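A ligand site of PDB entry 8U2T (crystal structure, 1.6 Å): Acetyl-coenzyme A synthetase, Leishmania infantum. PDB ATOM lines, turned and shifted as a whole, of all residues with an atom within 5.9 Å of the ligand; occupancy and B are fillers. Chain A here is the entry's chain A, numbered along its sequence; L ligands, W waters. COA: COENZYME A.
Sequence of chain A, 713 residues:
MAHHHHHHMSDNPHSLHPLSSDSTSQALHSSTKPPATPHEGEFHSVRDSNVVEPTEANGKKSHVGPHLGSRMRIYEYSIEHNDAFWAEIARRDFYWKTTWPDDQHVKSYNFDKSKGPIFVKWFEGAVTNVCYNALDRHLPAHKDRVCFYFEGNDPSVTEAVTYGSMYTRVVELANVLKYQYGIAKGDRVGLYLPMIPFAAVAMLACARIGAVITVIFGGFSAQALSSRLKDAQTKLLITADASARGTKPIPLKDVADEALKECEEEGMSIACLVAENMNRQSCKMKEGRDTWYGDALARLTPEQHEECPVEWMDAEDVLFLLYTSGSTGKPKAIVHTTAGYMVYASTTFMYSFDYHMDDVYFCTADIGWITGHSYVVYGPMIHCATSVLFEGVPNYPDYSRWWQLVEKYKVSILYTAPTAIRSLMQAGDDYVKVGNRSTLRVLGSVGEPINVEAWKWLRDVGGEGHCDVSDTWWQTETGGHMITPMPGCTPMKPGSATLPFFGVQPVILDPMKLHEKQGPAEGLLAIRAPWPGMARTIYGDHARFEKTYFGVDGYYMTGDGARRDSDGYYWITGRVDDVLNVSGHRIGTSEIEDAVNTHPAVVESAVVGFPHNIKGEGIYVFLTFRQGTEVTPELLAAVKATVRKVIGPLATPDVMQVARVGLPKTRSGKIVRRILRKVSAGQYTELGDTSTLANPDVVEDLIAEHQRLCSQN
The guanidinium group of Arg 644 is in salt-bridge range of an oxygen (O8A) of the ligand (2.7 Å). The guanidinium group (NE) of Arg 245 lies within salt-bridge range of an oxygen (O4A) of the ligand (2.8 Å). The side-chain amino group (NZ) of Lys 248 lies within salt-bridge range of an oxygen (O8A) of the ligand (2.8 Å). The side-chain carboxylate (OD2) of Asp 366 lies within hydrogen-bond range of a nitrogen (N6A) of the ligand (3.5 Å).
Merely in contact with the ligand: Phe 217 (3.4 Å), Pro 649 (3.5 Å), Gly 219 (3.5 Å), Gly 218 (3.6 Å), Val 393 (3.8 Å) and Ile 250 (3.9 Å). Hydrophobic or aromatic side chains that line the ligand: Phe 217, Ile 250, Val 393 and Pro 649. Ten residues have an atom within 4 Å of the ligand: Phe 217, Gly 218, Gly 219, Arg 245, Lys 248, Ile 250, Asp 366, Val 393, Arg 644 and Pro 649. The nearest printed residue that does not touch the ligand is Leu 650 (4.4 Å).
The guanidinium group of Arg 644 lies within hydrogen-bond range of the side-chain hydroxyl of Thr 652, at 2.8 Å. The backbone carbonyl oxygen (O) of Pro 649 sits at hydrogen-bond distance from the side-chain hydroxyl (OG1) of Thr 652, at 2.6 Å.
Water W1 bridges a nitrogen (N3A) of the ligand (2.7 Å) and the side-chain amino group of Lys 248 (3.1 Å). Water W4 bridges N7A of the ligand (2.9 Å) and NH2 of Arg 245 (3.3 Å). Water W2 bridges OD2 of Asp 366 and N6A of the ligand.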
ATOM      1  N   PHE A 217     -14.456   8.542 -27.575  1.00  0.00           N
ATOM      2  CA  PHE A 217     -14.274   9.829 -26.910  1.00  0.00           C
ATOM      3  C   PHE A 217     -14.761   9.765 -25.464  1.00  0.00           C
ATOM      4  O   PHE A 217     -15.871   9.297 -25.172  1.00  0.00           O
ATOM      5  CB  PHE A 217     -15.022  10.888 -27.714  1.00  0.00           C
ATOM      6  CG  PHE A 217     -15.109  12.257 -27.083  1.00  0.00           C
ATOM      7  CD1 PHE A 217     -13.966  13.009 -26.818  1.00  0.00           C
ATOM      8  CD2 PHE A 217     -16.358  12.811 -26.806  1.00  0.00           C
ATOM      9  CE1 PHE A 217     -14.070  14.266 -26.287  1.00  0.00           C
ATOM     10  CE2 PHE A 217     -16.457  14.102 -26.240  1.00  0.00           C
ATOM     11  CZ  PHE A 217     -15.316  14.813 -25.998  1.00  0.00           C
ATOM     12  N   GLY A 218     -13.927  10.248 -24.554  1.00  0.00           N
ATOM     13  CA  GLY A 218     -14.210  10.158 -23.125  1.00  0.00           C
ATOM     14  C   GLY A 218     -15.432  10.939 -22.667  1.00  0.00           C
ATOM     15  O   GLY A 218     -15.898  10.724 -21.548  1.00  0.00           O
ATOM     16  N   GLY A 219     -15.967  11.821 -23.509  1.00  0.00           N
ATOM     17  CA  GLY A 219     -17.185  12.512 -23.170  1.00  0.00           C
ATOM     18  C   GLY A 219     -18.467  11.799 -23.532  1.00  0.00           C
ATOM     19  O   GLY A 219     -19.549  12.258 -23.182  1.00  0.00           O
ATOM     20  N   PHE A 220     -18.391  10.693 -24.271  1.00  0.00           N
ATOM     21  CA  PHE A 220     -19.575   9.873 -24.503  1.00  0.00           C
ATOM     22  C   PHE A 220     -20.067   9.246 -23.200  1.00  0.00           C
ATOM     23  O   PHE A 220     -19.284   8.951 -22.282  1.00  0.00           O
ATOM     24  CB  PHE A 220     -19.293   8.790 -25.526  1.00  0.00           C
ATOM     25  CG  PHE A 220     -19.360   9.258 -26.955  1.00  0.00           C
ATOM     26  CD1 PHE A 220     -20.535   9.792 -27.459  1.00  0.00           C
ATOM     27  CD2 PHE A 220     -18.269   9.143 -27.783  1.00  0.00           C
ATOM     28  CE1 PHE A 220     -20.608  10.216 -28.752  1.00  0.00           C
ATOM     29  CE2 PHE A 220     -18.331   9.583 -29.087  1.00  0.00           C
ATOM     30  CZ  PHE A 220     -19.488  10.110 -29.576  1.00  0.00           C
ATOM     31  N   ARG A 245     -11.622  17.785 -15.813  1.00  0.00           N
ATOM     32  CA  ARG A 245     -11.684  18.779 -16.884  1.00  0.00           C
ATOM     33  C   ARG A 245     -12.065  20.087 -16.216  1.00  0.00           C
ATOM     34  O   ARG A 245     -13.242  20.314 -15.946  1.00  0.00           O
ATOM     35  CB  ARG A 245     -12.685  18.361 -17.942  1.00  0.00           C
ATOM     36  CG  ARG A 245     -12.602  19.155 -19.196  1.00  0.00           C
ATOM     37  CD  ARG A 245     -13.358  18.510 -20.357  1.00  0.00           C
ATOM     38  NE  ARG A 245     -13.108  19.269 -21.580  1.00  0.00           N
ATOM     39  CZ  ARG A 245     -12.056  19.104 -22.358  1.00  0.00           C
ATOM     40  NH1 ARG A 245     -11.133  18.180 -22.094  1.00  0.00           N
ATOM     41  NH2 ARG A 245     -11.911  19.883 -23.429  1.00  0.00           N
ATOM     42  N   LYS A 248     -14.574  19.909 -13.238  1.00  0.00           N
ATOM     43  CA  LYS A 248     -15.521  18.807 -13.408  1.00  0.00           C
ATOM     44  C   LYS A 248     -14.801  17.474 -13.275  1.00  0.00           C
ATOM     45  O   LYS A 248     -13.882  17.206 -14.064  1.00  0.00           O
ATOM     46  CB  LYS A 248     -16.216  18.891 -14.760  1.00  0.00           C
ATOM     47  CG  LYS A 248     -17.259  17.784 -14.979  1.00  0.00           C
ATOM     48  CD  LYS A 248     -17.929  17.859 -16.343  1.00  0.00           C
ATOM     49  CE  LYS A 248     -18.875  16.669 -16.547  1.00  0.00           C
ATOM     50  NZ  LYS A 248     -19.666  16.750 -17.829  1.00  0.00           N
ATOM     51  N   ILE A 250     -14.259  13.724 -14.182  1.00  0.00           N
ATOM     52  CA  ILE A 250     -14.596  12.916 -15.351  1.00  0.00           C
ATOM     53  C   ILE A 250     -14.537  11.448 -14.954  1.00  0.00           C
ATOM     54  O   ILE A 250     -13.458  10.838 -14.993  1.00  0.00           O
ATOM     55  CB  ILE A 250     -13.665  13.187 -16.534  1.00  0.00           C
ATOM     56  CG1 ILE A 250     -13.659  14.691 -16.896  1.00  0.00           C
ATOM     57  CG2 ILE A 250     -14.069  12.324 -17.731  1.00  0.00           C
ATOM     58  CD1 ILE A 250     -15.028  15.283 -17.243  1.00  0.00           C
ATOM     59  N   ASP A 366      -8.699  15.887 -29.178  1.00  0.00           N
ATOM     60  CA  ASP A 366      -8.787  14.634 -28.446  1.00  0.00           C
ATOM     61  C   ASP A 366      -8.584  13.440 -29.365  1.00  0.00           C
ATOM     62  O   ASP A 366      -8.981  13.461 -30.539  1.00  0.00           O
ATOM     63  CB  ASP A 366     -10.162  14.557 -27.777  1.00  0.00           C
ATOM     64  CG  ASP A 366     -10.244  13.501 -26.698  1.00  0.00           C
ATOM     65  OD1 ASP A 366     -10.537  12.335 -27.032  1.00  0.00           O
ATOM     66  OD2 ASP A 366     -10.018  13.848 -25.507  1.00  0.00           O
ATOM     67  N   VAL A 393      -8.084  21.765 -20.123  1.00  0.00           N
ATOM     68  CA  VAL A 393      -8.951  22.660 -20.892  1.00  0.00           C
ATOM     69  C   VAL A 393      -8.316  24.042 -20.932  1.00  0.00           C
ATOM     70  O   VAL A 393      -7.593  24.392 -19.989  1.00  0.00           O
ATOM     71  CB  VAL A 393     -10.359  22.757 -20.291  1.00  0.00           C
ATOM     72  CG1 VAL A 393     -11.117  21.526 -20.582  1.00  0.00           C
ATOM     73  CG2 VAL A 393     -10.285  23.012 -18.779  1.00  0.00           C
ATOM     74  N   PRO A 394      -8.610  24.847 -21.966  1.00  0.00           N
ATOM     75  CA  PRO A 394      -7.947  26.175 -22.078  1.00  0.00           C
ATOM     76  C   PRO A 394      -8.297  27.165 -20.987  1.00  0.00           C
ATOM     77  O   PRO A 394      -7.624  28.201 -20.900  1.00  0.00           O
ATOM     78  CB  PRO A 394      -8.424  26.685 -23.445  1.00  0.00           C
ATOM     79  CG  PRO A 394      -9.679  25.911 -23.757  1.00  0.00           C
ATOM     80  CD  PRO A 394      -9.466  24.554 -23.123  1.00  0.00           C
ATOM     81  N   ASN A 395      -9.307  26.924 -20.151  1.00  0.00           N
ATOM     82  CA  ASN A 395      -9.700  27.936 -19.161  1.00  0.00           C
ATOM     83  C   ASN A 395      -9.436  27.509 -17.717  1.00  0.00           C
ATOM     84  O   ASN A 395     -10.050  28.082 -16.802  1.00  0.00           O
ATOM     85  CB  ASN A 395     -11.172  28.317 -19.336  1.00  0.00           C
ATOM     86  CG  ASN A 395     -12.104  27.228 -18.847  1.00  0.00           C
ATOM     87  OD1 ASN A 395     -11.837  26.047 -19.029  1.00  0.00           O
ATOM     88  ND2 ASN A 395     -13.189  27.628 -18.202  1.00  0.00           N
ATOM     89  N   SER A 583     -19.393  22.797 -32.301  1.00  0.00           N
ATOM     90  CA  SER A 583     -18.077  22.981 -31.671  1.00  0.00           C
ATOM     91  C   SER A 583     -17.032  22.080 -32.313  1.00  0.00           C
ATOM     92  O   SER A 583     -16.152  21.544 -31.646  1.00  0.00           O
ATOM     93  CB  SER A 583     -18.146  22.716 -30.162  1.00  0.00           C
ATOM     94  OG  SER A 583     -19.087  23.555 -29.528  1.00  0.00           O
ATOM     95  N   HIS A 585     -17.604  19.141 -33.603  1.00  0.00           N
ATOM     96  CA  HIS A 585     -18.024  17.746 -33.542  1.00  0.00           C
ATOM     97  C   HIS A 585     -19.224  17.531 -34.459  1.00  0.00           C
ATOM     98  O   HIS A 585     -20.208  18.286 -34.398  1.00  0.00           O
ATOM     99  CB  HIS A 585     -18.379  17.356 -32.102  1.00  0.00           C
ATOM    100  CG  HIS A 585     -17.331  17.732 -31.107  1.00  0.00           C
ATOM    101  ND1 HIS A 585     -15.985  17.521 -31.327  1.00  0.00           N
ATOM    102  CD2 HIS A 585     -17.419  18.302 -29.880  1.00  0.00           C
ATOM    103  CE1 HIS A 585     -15.300  17.941 -30.274  1.00  0.00           C
ATOM    104  NE2 HIS A 585     -16.146  18.419 -29.386  1.00  0.00           N
ATOM    105  N   LYS A 615     -20.087  28.203 -30.856  1.00  0.00           N
ATOM    106  CA  LYS A 615     -20.072  26.803 -31.256  1.00  0.00           C
ATOM    107  C   LYS A 615     -20.168  26.609 -32.760  1.00  0.00           C
ATOM    108  O   LYS A 615     -20.049  25.471 -33.227  1.00  0.00           O
ATOM    109  CB  LYS A 615     -21.223  26.051 -30.568  1.00  0.00           C
ATOM    110  CG  LYS A 615     -21.346  26.380 -29.081  1.00  0.00           C
ATOM    111  CD  LYS A 615     -21.512  25.170 -28.183  1.00  0.00           C
ATOM    112  CE  LYS A 615     -22.969  24.777 -28.032  1.00  0.00           C
ATOM    113  NZ  LYS A 615     -23.120  23.692 -26.999  1.00  0.00           N
ATOM    114  N   ARG A 644     -28.188  13.796 -22.642  1.00  0.00           N
ATOM    115  CA  ARG A 644     -26.828  13.618 -22.149  1.00  0.00           C
ATOM    116  C   ARG A 644     -26.593  12.206 -21.621  1.00  0.00           C
ATOM    117  O   ARG A 644     -25.446  11.720 -21.677  1.00  0.00           O
ATOM    118  CB  ARG A 644     -26.548  14.678 -21.080  1.00  0.00           C
ATOM    119  CG  ARG A 644     -26.560  16.078 -21.665  1.00  0.00           C
ATOM    120  CD  ARG A 644     -26.603  17.152 -20.601  1.00  0.00           C
ATOM    121  NE  ARG A 644     -25.502  17.044 -19.662  1.00  0.00           N
ATOM    122  CZ  ARG A 644     -24.395  17.782 -19.672  1.00  0.00           C
ATOM    123  NH1 ARG A 644     -24.152  18.638 -20.644  1.00  0.00           N
ATOM    124  NH2 ARG A 644     -23.518  17.653 -18.679  1.00  0.00           N
ATOM    125  N   PRO A 649     -22.625  14.782 -23.051  1.00  0.00           N
ATOM    126  CA  PRO A 649     -22.704  16.254 -22.994  1.00  0.00           C
ATOM    127  C   PRO A 649     -22.493  16.971 -24.313  1.00  0.00           C
ATOM    128  O   PRO A 649     -23.034  18.084 -24.500  1.00  0.00           O
ATOM    129  CB  PRO A 649     -21.600  16.604 -21.988  1.00  0.00           C
ATOM    130  CG  PRO A 649     -21.531  15.451 -21.102  1.00  0.00           C
ATOM    131  CD  PRO A 649     -21.787  14.247 -21.974  1.00  0.00           C
ATOM    132  N   LEU A 650     -21.741  16.382 -25.244  1.00  0.00           N
ATOM    133  CA  LEU A 650     -21.537  17.051 -26.521  1.00  0.00           C
ATOM    134  C   LEU A 650     -22.841  17.275 -27.266  1.00  0.00           C
ATOM    135  O   LEU A 650     -22.908  18.172 -28.113  1.00  0.00           O
ATOM    136  CB  LEU A 650     -20.565  16.244 -27.399  1.00  0.00           C
ATOM    137  CG  LEU A 650     -20.999  14.904 -28.018  1.00  0.00           C
ATOM    138  CD1 LEU A 650     -19.929  14.414 -28.987  1.00  0.00           C
ATOM    139  CD2 LEU A 650     -21.247  13.801 -26.959  1.00  0.00           C
ATOM    140  N   THR A 652     -25.781  18.124 -25.894  1.00  0.00           N
ATOM    141  CA  THR A 652     -26.718  18.899 -25.088  1.00  0.00           C
ATOM    142  C   THR A 652     -27.442  19.933 -25.946  1.00  0.00           C
ATOM    143  O   THR A 652     -26.795  20.732 -26.625  1.00  0.00           O
ATOM    144  CB  THR A 652     -25.994  19.634 -23.959  1.00  0.00           C
ATOM    145  OG1 THR A 652     -25.225  18.713 -23.183  1.00  0.00           O
ATOM    146  CG2 THR A 652     -26.982  20.330 -23.039  1.00  0.00           C
HETATM  147  N1A COA L   1     -13.923  14.070 -21.665  1.00  0.00           N
HETATM  148  C2A COA L   1     -15.060  14.214 -20.974  1.00  0.00           C
HETATM  149  N3A COA L   1     -15.978  15.173 -21.060  1.00  0.00           N
HETATM  150  C4A COA L   1     -15.647  16.072 -22.000  1.00  0.00           C
HETATM  151  C5A COA L   1     -14.512  16.063 -22.790  1.00  0.00           C
HETATM  152  C6A COA L   1     -13.606  14.993 -22.604  1.00  0.00           C
HETATM  153  N6A COA L   1     -12.466  14.866 -23.277  1.00  0.00           N
HETATM  154  N7A COA L   1     -14.511  17.164 -23.642  1.00  0.00           N
HETATM  155  C8A COA L   1     -15.626  17.798 -23.384  1.00  0.00           C
HETATM  156  N9A COA L   1     -16.363  17.175 -22.393  1.00  0.00           N
HETATM  157  C1B COA L   1     -17.627  17.644 -21.806  1.00  0.00           C
HETATM  158  C2B COA L   1     -17.402  18.917 -20.995  1.00  0.00           C
HETATM  159  O2B COA L   1     -16.941  18.607 -19.703  1.00  0.00           O
HETATM  160  C3B COA L   1     -18.789  19.554 -21.033  1.00  0.00           C
HETATM  161  O3B COA L   1     -19.572  18.951 -20.007  1.00  0.00           O
HETATM  162  P3B COA L   1     -20.686  19.906 -19.306  1.00  0.00           P
HETATM  163  O7A COA L   1     -20.030  21.195 -18.791  1.00  0.00           O
HETATM  164  O8A COA L   1     -21.240  19.080 -18.182  1.00  0.00           O
HETATM  165  O9A COA L   1     -21.709  20.200 -20.380  1.00  0.00           O
HETATM  166  C4B COA L   1     -19.287  19.181 -22.426  1.00  0.00           C
HETATM  167  O4B COA L   1     -18.507  18.020 -22.834  1.00  0.00           O
HETATM  168  C5B COA L   1     -19.102  20.254 -23.475  1.00  0.00           C
HETATM  169  O5B COA L   1     -17.704  20.446 -23.725  1.00  0.00           O
HETATM  170  P1A COA L   1     -17.309  21.701 -24.640  1.00  0.00           P
HETATM  171  O1A COA L   1     -18.209  22.853 -24.302  1.00  0.00           O
HETATM  172  O2A COA L   1     -17.173  21.277 -26.058  1.00  0.00           O
HETATM  173  O3A COA L   1     -15.867  22.060 -24.041  1.00  0.00           O
HETATM  174  P2A COA L   1     -15.596  22.539 -22.544  1.00  0.00           P
HETATM  175  O4A COA L   1     -14.700  21.544 -21.883  1.00  0.00           O
HETATM  176  O5A COA L   1     -16.915  22.859 -21.917  1.00  0.00           O
HETATM  177  O6A COA L   1     -14.799  23.921 -22.775  1.00  0.00           O
HETATM  178  O   HOH W   1     -18.144  14.676 -19.511  1.00  0.00           O
HETATM  179  O   HOH W   2     -10.169  13.019 -23.159  1.00  0.00           O
HETATM  180  O   HOH W   3     -11.771  12.435 -20.995  1.00  0.00           O
HETATM  181  O   HOH W   4     -12.459  17.522 -25.683  1.00  0.00           O
HETATM  182  O   HOH W   5     -22.150  20.738 -24.366  1.00  0.00           O
